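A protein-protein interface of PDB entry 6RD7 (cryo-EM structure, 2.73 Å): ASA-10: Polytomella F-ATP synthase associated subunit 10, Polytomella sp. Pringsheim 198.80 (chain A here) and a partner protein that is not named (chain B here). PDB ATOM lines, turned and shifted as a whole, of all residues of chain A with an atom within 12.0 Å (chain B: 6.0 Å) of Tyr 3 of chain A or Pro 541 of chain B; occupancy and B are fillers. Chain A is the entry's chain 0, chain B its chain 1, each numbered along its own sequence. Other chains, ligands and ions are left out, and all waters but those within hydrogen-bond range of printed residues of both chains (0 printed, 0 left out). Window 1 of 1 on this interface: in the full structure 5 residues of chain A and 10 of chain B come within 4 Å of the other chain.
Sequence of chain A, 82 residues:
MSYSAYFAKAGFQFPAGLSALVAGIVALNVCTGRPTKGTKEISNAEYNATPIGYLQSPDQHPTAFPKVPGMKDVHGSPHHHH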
ATOM      1  N   MET A   1       7.330  10.549   9.379  1.00  0.00           N
ATOM      2  CA  MET A   1       7.431   9.440   8.440  1.00  0.00           C
ATOM      3  C   MET A   1       8.563   9.747   7.455  1.00  0.00           C
ATOM      4  O   MET A   1       8.897  10.905   7.224  1.00  0.00           O
ATOM      5  CB  MET A   1       6.079   9.205   7.748  1.00  0.00           C
ATOM      6  CG  MET A   1       5.966   7.943   6.899  1.00  0.00           C
ATOM      7  SD  MET A   1       6.253   6.378   7.732  1.00  0.00           S
ATOM      8  CE  MET A   1       6.712   5.363   6.326  1.00  0.00           C
ATOM      9  N   SER A   2       9.164   8.694   6.905  1.00  0.00           N
ATOM     10  CA  SER A   2      10.437   8.785   6.208  1.00  0.00           C
ATOM     11  C   SER A   2      10.337   8.274   4.780  1.00  0.00           C
ATOM     12  O   SER A   2       9.295   7.763   4.368  1.00  0.00           O
ATOM     13  CB  SER A   2      11.487   7.983   6.974  1.00  0.00           C
ATOM     14  OG  SER A   2      11.210   6.597   6.882  1.00  0.00           O
ATOM     15  N   TYR A   3      11.418   8.404   4.016  1.00  0.00           N
ATOM     16  CA  TYR A   3      11.520   7.777   2.709  1.00  0.00           C
ATOM     17  C   TYR A   3      12.216   6.429   2.774  1.00  0.00           C
ATOM     18  O   TYR A   3      12.697   5.945   1.749  1.00  0.00           O
ATOM     19  CB  TYR A   3      12.269   8.681   1.734  1.00  0.00           C
ATOM     20  CG  TYR A   3      11.547   9.934   1.323  1.00  0.00           C
ATOM     21  CD1 TYR A   3      10.519   9.891   0.398  1.00  0.00           C
ATOM     22  CD2 TYR A   3      11.913  11.168   1.837  1.00  0.00           C
ATOM     23  CE1 TYR A   3       9.865  11.037   0.011  1.00  0.00           C
ATOM     24  CE2 TYR A   3      11.264  12.319   1.453  1.00  0.00           C
ATOM     25  CZ  TYR A   3      10.242  12.245   0.540  1.00  0.00           C
ATOM     26  OH  TYR A   3       9.585  13.384   0.151  1.00  0.00           O
ATOM     27  N   SER A   4      12.284   5.819   3.959  1.00  0.00           N
ATOM     28  CA  SER A   4      13.043   4.586   4.138  1.00  0.00           C
ATOM     29  C   SER A   4      12.369   3.411   3.446  1.00  0.00           C
ATOM     30  O   SER A   4      13.038   2.551   2.863  1.00  0.00           O
ATOM     31  CB  SER A   4      13.210   4.295   5.627  1.00  0.00           C
ATOM     32  OG  SER A   4      14.061   5.243   6.236  1.00  0.00           O
ATOM     33  N   ALA A   5      11.038   3.357   3.505  1.00  0.00           N
ATOM     34  CA  ALA A   5      10.314   2.255   2.886  1.00  0.00           C
ATOM     35  C   ALA A   5      10.348   2.358   1.369  1.00  0.00           C
ATOM     36  O   ALA A   5      10.331   1.337   0.668  1.00  0.00           O
ATOM     37  CB  ALA A   5       8.877   2.227   3.393  1.00  0.00           C
ATOM     38  N   TYR A   6      10.418   3.583   0.848  1.00  0.00           N
ATOM     39  CA  TYR A   6      10.519   3.788  -0.592  1.00  0.00           C
ATOM     40  C   TYR A   6      11.849   3.275  -1.125  1.00  0.00           C
ATOM     41  O   TYR A   6      11.925   2.750  -2.241  1.00  0.00           O
ATOM     42  CB  TYR A   6      10.341   5.272  -0.914  1.00  0.00           C
ATOM     43  CG  TYR A   6      10.796   5.663  -2.294  1.00  0.00           C
ATOM     44  CD1 TYR A   6      10.056   5.310  -3.411  1.00  0.00           C
ATOM     45  CD2 TYR A   6      11.963   6.388  -2.483  1.00  0.00           C
ATOM     46  CE1 TYR A   6      10.466   5.662  -4.674  1.00  0.00           C
ATOM     47  CE2 TYR A   6      12.382   6.740  -3.740  1.00  0.00           C
ATOM     48  CZ  TYR A   6      11.630   6.377  -4.833  1.00  0.00           C
ATOM     49  OH  TYR A   6      12.043   6.732  -6.093  1.00  0.00           O
ATOM     50  N   PHE A   7      12.912   3.410  -0.334  1.00  0.00           N
ATOM     51  CA  PHE A   7      14.208   2.902  -0.763  1.00  0.00           C
ATOM     52  C   PHE A   7      14.350   1.425  -0.446  1.00  0.00           C
ATOM     53  O   PHE A   7      15.173   0.731  -1.050  1.00  0.00           O
ATOM     54  CB  PHE A   7      15.326   3.712  -0.118  1.00  0.00           C
ATOM     55  CG  PHE A   7      15.506   5.046  -0.739  1.00  0.00           C
ATOM     56  CD1 PHE A   7      15.777   5.149  -2.089  1.00  0.00           C
ATOM     57  CD2 PHE A   7      15.363   6.196   0.004  1.00  0.00           C
ATOM     58  CE1 PHE A   7      15.921   6.373  -2.678  1.00  0.00           C
ATOM     59  CE2 PHE A   7      15.506   7.421  -0.582  1.00  0.00           C
ATOM     60  CZ  PHE A   7      15.780   7.507  -1.923  1.00  0.00           C
ATOM     61  N   ALA A   8      13.553   0.924   0.497  1.00  0.00           N
ATOM     62  CA  ALA A   8      13.518  -0.513   0.731  1.00  0.00           C
ATOM     63  C   ALA A   8      12.733  -1.233  -0.354  1.00  0.00           C
ATOM     64  O   ALA A   8      12.904  -2.442  -0.538  1.00  0.00           O
ATOM     65  CB  ALA A   8      12.924  -0.805   2.105  1.00  0.00           C
ATOM     66  N   LYS A   9      11.861  -0.514  -1.070  1.00  0.00           N
ATOM     67  CA  LYS A   9      11.116  -1.124  -2.170  1.00  0.00           C
ATOM     68  C   LYS A   9      12.031  -1.515  -3.321  1.00  0.00           C
ATOM     69  O   LYS A   9      11.813  -2.541  -3.974  1.00  0.00           O
ATOM     70  CB  LYS A   9      10.041  -0.171  -2.681  1.00  0.00           C
ATOM     71  CG  LYS A   9       8.785  -0.125  -1.856  1.00  0.00           C
ATOM     72  CD  LYS A   9       7.861   0.942  -2.397  1.00  0.00           C
ATOM     73  CE  LYS A   9       7.069   1.588  -1.291  1.00  0.00           C
ATOM     74  NZ  LYS A   9       5.628   1.233  -1.350  1.00  0.00           N
ATOM     75  N   ALA A  10      13.043  -0.702  -3.601  1.00  0.00           N
ATOM     76  CA  ALA A  10      13.953  -0.998  -4.697  1.00  0.00           C
ATOM     77  C   ALA A  10      14.895  -2.125  -4.302  1.00  0.00           C
ATOM     78  O   ALA A  10      15.534  -2.077  -3.246  1.00  0.00           O
ATOM     79  CB  ALA A  10      14.746   0.249  -5.081  1.00  0.00           C
ATOM     80  N   GLY A  11      14.981  -3.143  -5.150  1.00  0.00           N
ATOM     81  CA  GLY A  11      15.831  -4.275  -4.862  1.00  0.00           C
ATOM     82  C   GLY A  11      17.292  -3.995  -5.135  1.00  0.00           C
ATOM     83  O   GLY A  11      17.723  -2.855  -5.307  1.00  0.00           O
ATOM     84  N   PRO B 319      17.518   4.682   5.980  1.00  0.00           N
ATOM     85  CA  PRO B 319      17.810   3.296   5.571  1.00  0.00           C
ATOM     86  C   PRO B 319      19.189   2.800   5.963  1.00  0.00           C
ATOM     87  O   PRO B 319      19.365   1.587   6.129  1.00  0.00           O
ATOM     88  CB  PRO B 319      17.663   3.340   4.046  1.00  0.00           C
ATOM     89  CG  PRO B 319      16.796   4.473   3.779  1.00  0.00           C
ATOM     90  CD  PRO B 319      17.065   5.487   4.830  1.00  0.00           C
ATOM     91  N   HIS B 531      11.104  21.130   3.451  1.00  0.00           N
ATOM     92  CA  HIS B 531      11.159  19.701   3.158  1.00  0.00           C
ATOM     93  C   HIS B 531      12.565  19.255   2.775  1.00  0.00           C
ATOM     94  O   HIS B 531      13.017  18.182   3.210  1.00  0.00           O
ATOM     95  CB  HIS B 531      10.177  19.358   2.046  1.00  0.00           C
ATOM     96  CG  HIS B 531      10.042  17.891   1.794  1.00  0.00           C
ATOM     97  ND1 HIS B 531       9.348  17.054   2.637  1.00  0.00           N
ATOM     98  CD2 HIS B 531      10.513  17.112   0.795  1.00  0.00           C
ATOM     99  CE1 HIS B 531       9.395  15.822   2.166  1.00  0.00           C
ATOM    100  NE2 HIS B 531      10.094  15.830   1.048  1.00  0.00           N
ATOM    101  N   HIS B 535      14.994  16.672   4.971  1.00  0.00           N
ATOM    102  CA  HIS B 535      15.350  15.350   4.478  1.00  0.00           C
ATOM    103  C   HIS B 535      16.702  15.243   3.783  1.00  0.00           C
ATOM    104  O   HIS B 535      17.124  14.118   3.504  1.00  0.00           O
ATOM    105  CB  HIS B 535      14.260  14.839   3.533  1.00  0.00           C
ATOM    106  CG  HIS B 535      12.997  14.456   4.233  1.00  0.00           C
ATOM    107  ND1 HIS B 535      12.846  13.253   4.884  1.00  0.00           N
ATOM    108  CD2 HIS B 535      11.832  15.120   4.396  1.00  0.00           C
ATOM    109  CE1 HIS B 535      11.638  13.191   5.411  1.00  0.00           C
ATOM    110  NE2 HIS B 535      11.003  14.311   5.130  1.00  0.00           N
ATOM    111  N   ASP B 539      17.474  10.877   3.920  1.00  0.00           N
ATOM    112  CA  ASP B 539      16.727   9.955   3.078  1.00  0.00           C
ATOM    113  C   ASP B 539      16.057  10.615   1.882  1.00  0.00           C
ATOM    114  O   ASP B 539      15.181   9.996   1.281  1.00  0.00           O
ATOM    115  CB  ASP B 539      15.675   9.203   3.902  1.00  0.00           C
ATOM    116  CG  ASP B 539      14.741  10.128   4.654  1.00  0.00           C
ATOM    117  OD1 ASP B 539      15.003  11.342   4.714  1.00  0.00           O
ATOM    118  OD2 ASP B 539      13.736   9.632   5.196  1.00  0.00           O
ATOM    119  N   LEU B 540      16.422  11.837   1.527  1.00  0.00           N
ATOM    120  CA  LEU B 540      15.757  12.528   0.424  1.00  0.00           C
ATOM    121  C   LEU B 540      16.118  11.878  -0.901  1.00  0.00           C
ATOM    122  O   LEU B 540      17.306  11.708  -1.190  1.00  0.00           O
ATOM    123  CB  LEU B 540      16.150  13.998   0.405  1.00  0.00           C
ATOM    124  CG  LEU B 540      15.344  15.002  -0.418  1.00  0.00           C
ATOM    125  CD1 LEU B 540      13.860  14.827  -0.215  1.00  0.00           C
ATOM    126  CD2 LEU B 540      15.758  16.393  -0.028  1.00  0.00           C
ATOM    127  N   PRO B 541      15.150  11.466  -1.710  1.00  0.00           N
ATOM    128  CA  PRO B 541      15.474  10.943  -3.035  1.00  0.00           C
ATOM    129  C   PRO B 541      15.913  12.050  -3.972  1.00  0.00           C
ATOM    130  O   PRO B 541      15.571  13.220  -3.799  1.00  0.00           O
ATOM    131  CB  PRO B 541      14.152  10.322  -3.500  1.00  0.00           C
ATOM    132  CG  PRO B 541      13.349  10.157  -2.275  1.00  0.00           C
ATOM    133  CD  PRO B 541      13.727  11.286  -1.395  1.00  0.00           C
ATOM    134  N   HIS B 542      16.691  11.663  -4.980  1.00  0.00           N
ATOM    135  CA  HIS B 542      17.076  12.625  -6.003  1.00  0.00           C
ATOM    136  C   HIS B 542      15.901  12.971  -6.904  1.00  0.00           C
ATOM    137  O   HIS B 542      15.891  14.042  -7.519  1.00  0.00           O
ATOM    138  CB  HIS B 542      18.237  12.080  -6.828  1.00  0.00           C
ATOM    139  CG  HIS B 542      19.580  12.331  -6.220  1.00  0.00           C
ATOM    140  ND1 HIS B 542      20.531  13.121  -6.823  1.00  0.00           N
ATOM    141  CD2 HIS B 542      20.133  11.890  -5.068  1.00  0.00           C
ATOM    142  CE1 HIS B 542      21.612  13.161  -6.066  1.00  0.00           C
ATOM    143  NE2 HIS B 542      21.396  12.422  -4.995  1.00  0.00           N
ATOM    144  N   SER B 543      14.907  12.086  -6.988  1.00  0.00           N
ATOM    145  CA  SER B 543      13.723  12.363  -7.791  1.00  0.00           C
ATOM    146  C   SER B 543      12.875  13.454  -7.162  1.00  0.00           C
ATOM    147  O   SER B 543      12.318  14.298  -7.866  1.00  0.00           O
ATOM    148  CB  SER B 543      12.902  11.091  -7.962  1.00  0.00           C
ATOM    149  OG  SER B 543      12.695  10.453  -6.720  1.00  0.00           O
ATOM    150  N   VAL B 544      12.783  13.463  -5.833  1.00  0.00           N
ATOM    151  CA  VAL B 544      12.025  14.491  -5.131  1.00  0.00           C
ATOM    152  C   VAL B 544      12.741  15.833  -5.226  1.00  0.00           C
ATOM    153  O   VAL B 544      12.106  16.887  -5.351  1.00  0.00           O
ATOM    154  CB  VAL B 544      11.797  14.040  -3.677  1.00  0.00           C
ATOM    155  CG1 VAL B 544      11.011  15.049  -2.899  1.00  0.00           C
ATOM    156  CG2 VAL B 544      11.065  12.726  -3.667  1.00  0.00           C
ATOM    157  N   VAL B 545      14.074  15.806  -5.222  1.00  0.00           N
ATOM    158  CA  VAL B 545      14.875  17.012  -5.410  1.00  0.00           C
ATOM    159  C   VAL B 545      14.688  17.570  -6.815  1.00  0.00           C
ATOM    160  O   VAL B 545      14.463  18.771  -6.996  1.00  0.00           O
ATOM    161  CB  VAL B 545      16.354  16.700  -5.112  1.00  0.00           C
ATOM    162  CG1 VAL B 545      17.261  17.744  -5.697  1.00  0.00           C
ATOM    163  CG2 VAL B 545      16.577  16.599  -3.634  1.00  0.00           C
ATOM    164  N   ALA B 546      14.746  16.702  -7.827  1.00  0.00           N
ATOM    165  CA  ALA B 546      14.595  17.153  -9.207  1.00  0.00           C
ATOM    166  C   ALA B 546      13.158  17.551  -9.512  1.00  0.00           C
ATOM    167  O   ALA B 546      12.906  18.316 -10.447  1.00  0.00           O
ATOM    168  CB  ALA B 546      15.064  16.064 -10.165  1.00  0.00           C
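The backbone carbonyl oxygen of His 535 of chain B lies within hydrogen-bond range of the backbone NH of Leu 540 of chain B.
The backbone NH (N) of Ser 4 of chain A sits at hydrogen-bond distance from the side-chain hydroxyl (OG) of Ser 2 of chain A, at 3.2 Å.
The side-chain carboxylate of Asp 539 of chain B sits at hydrogen-bond distance from a ring nitrogen (ND1) of His 535 of chain B (2.9 Å).
Tyr 3 of chain A touches just these residues of chain B: His 531 (2.7 Å), His 535 (3.8 Å), Asp 539 (2.9 Å), Leu 540 (3.98 Å), Pro 541 (3.7 Å) and Val 544 (3.8 Å).
Of chain A, only Tyr 3, Tyr 6 and Phe 7 come within 4 Å of Pro 541 of chain B.
Of chain A, only Tyr 3 (3.98 Å) comes within 4 Å of Leu 540 of chain B.
No residue of chain A comes within 4 Å of His 542 of chain B.
Ser 543 of chain B touches just one residue of chain A: Tyr 6 (3.8 Å).
Val 544 of chain B touches just one residue of chain A: Tyr 3.
No residue of chain A comes within 4 Å of Val 545 of chain B.
Printed residues of chain B within 4 Å of Tyr 6 of chain A: Pro 541 and Ser 543.
Printed residues of chain B within 4 Å of Phe 7 of chain A: Asp 539 (3.2 Å) and Pro 541 (3.6 Å).
The nearest residue of chain B that does not touch Tyr 3 of chain A is Pro 319 of chain B (4.8 Å).
The nearest printed residue of chain A that does not touch Pro 541 of chain B is Ser 2 of chain A (7.7 Å).
Of the 11 printed residues of chain A, 5 touch a printed residue of chain B.
Hydrophobic or aromatic side chains of chain B within 4 Å of the printed part of chain A: Pro 319, His 531, His 535, Leu 540, Pro 541 and Val 544.
Along chain B the printed residues that touch a printed residue of chain A span positions 319 to 544.
Among the printed residues, no Asp or Glu carboxylate lies within 4 Å of a Lys or Arg side-chain nitrogen of the other chain.
CB of Ser 2 of chain A touches OD2 of Asp 539 of chain B (3.3 Å).
Tyr 3 of chain A touches His 535 of chain B.
Leu 540 of chain B touches Tyr 3 of chain A (CD1 to CE2, 3.98 Å).
CD of Pro 541 of chain B touches CD2 of Tyr 3 of chain A, at 3.7 Å.
OH of Tyr 3 of chain A touches CG1 of Val 544 of chain B, 3.8 Å away.
CD of Pro 319 of chain B touches OG of Ser 4 of chain A, at 3.3 Å.
CG of Pro 541 of chain B touches CE2 of Tyr 6 of chain A, at 3.8 Å.
Tyr 6 of chain A touches Ser 543 of chain B (OH to OG, 3.8 Å).
CE2 of Phe 7 of chain A touches O of Asp 539 of chain B, at 3.2 Å.
Pro 541 of chain B touches Phe 7 of chain A (CG to CZ, 3.6 Å).
The backbone NH (N) of Tyr 3 of chain A sits at hydrogen-bond distance from the side-chain carboxylate (OD2) of Asp 539 of chain B, 2.9 Å away.
A ring nitrogen (NE2) of His 531 of chain B is in hydrogen-bond range of the side-chain hydroxyl (OH) of Tyr 3 of chain A (2.7 Å).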
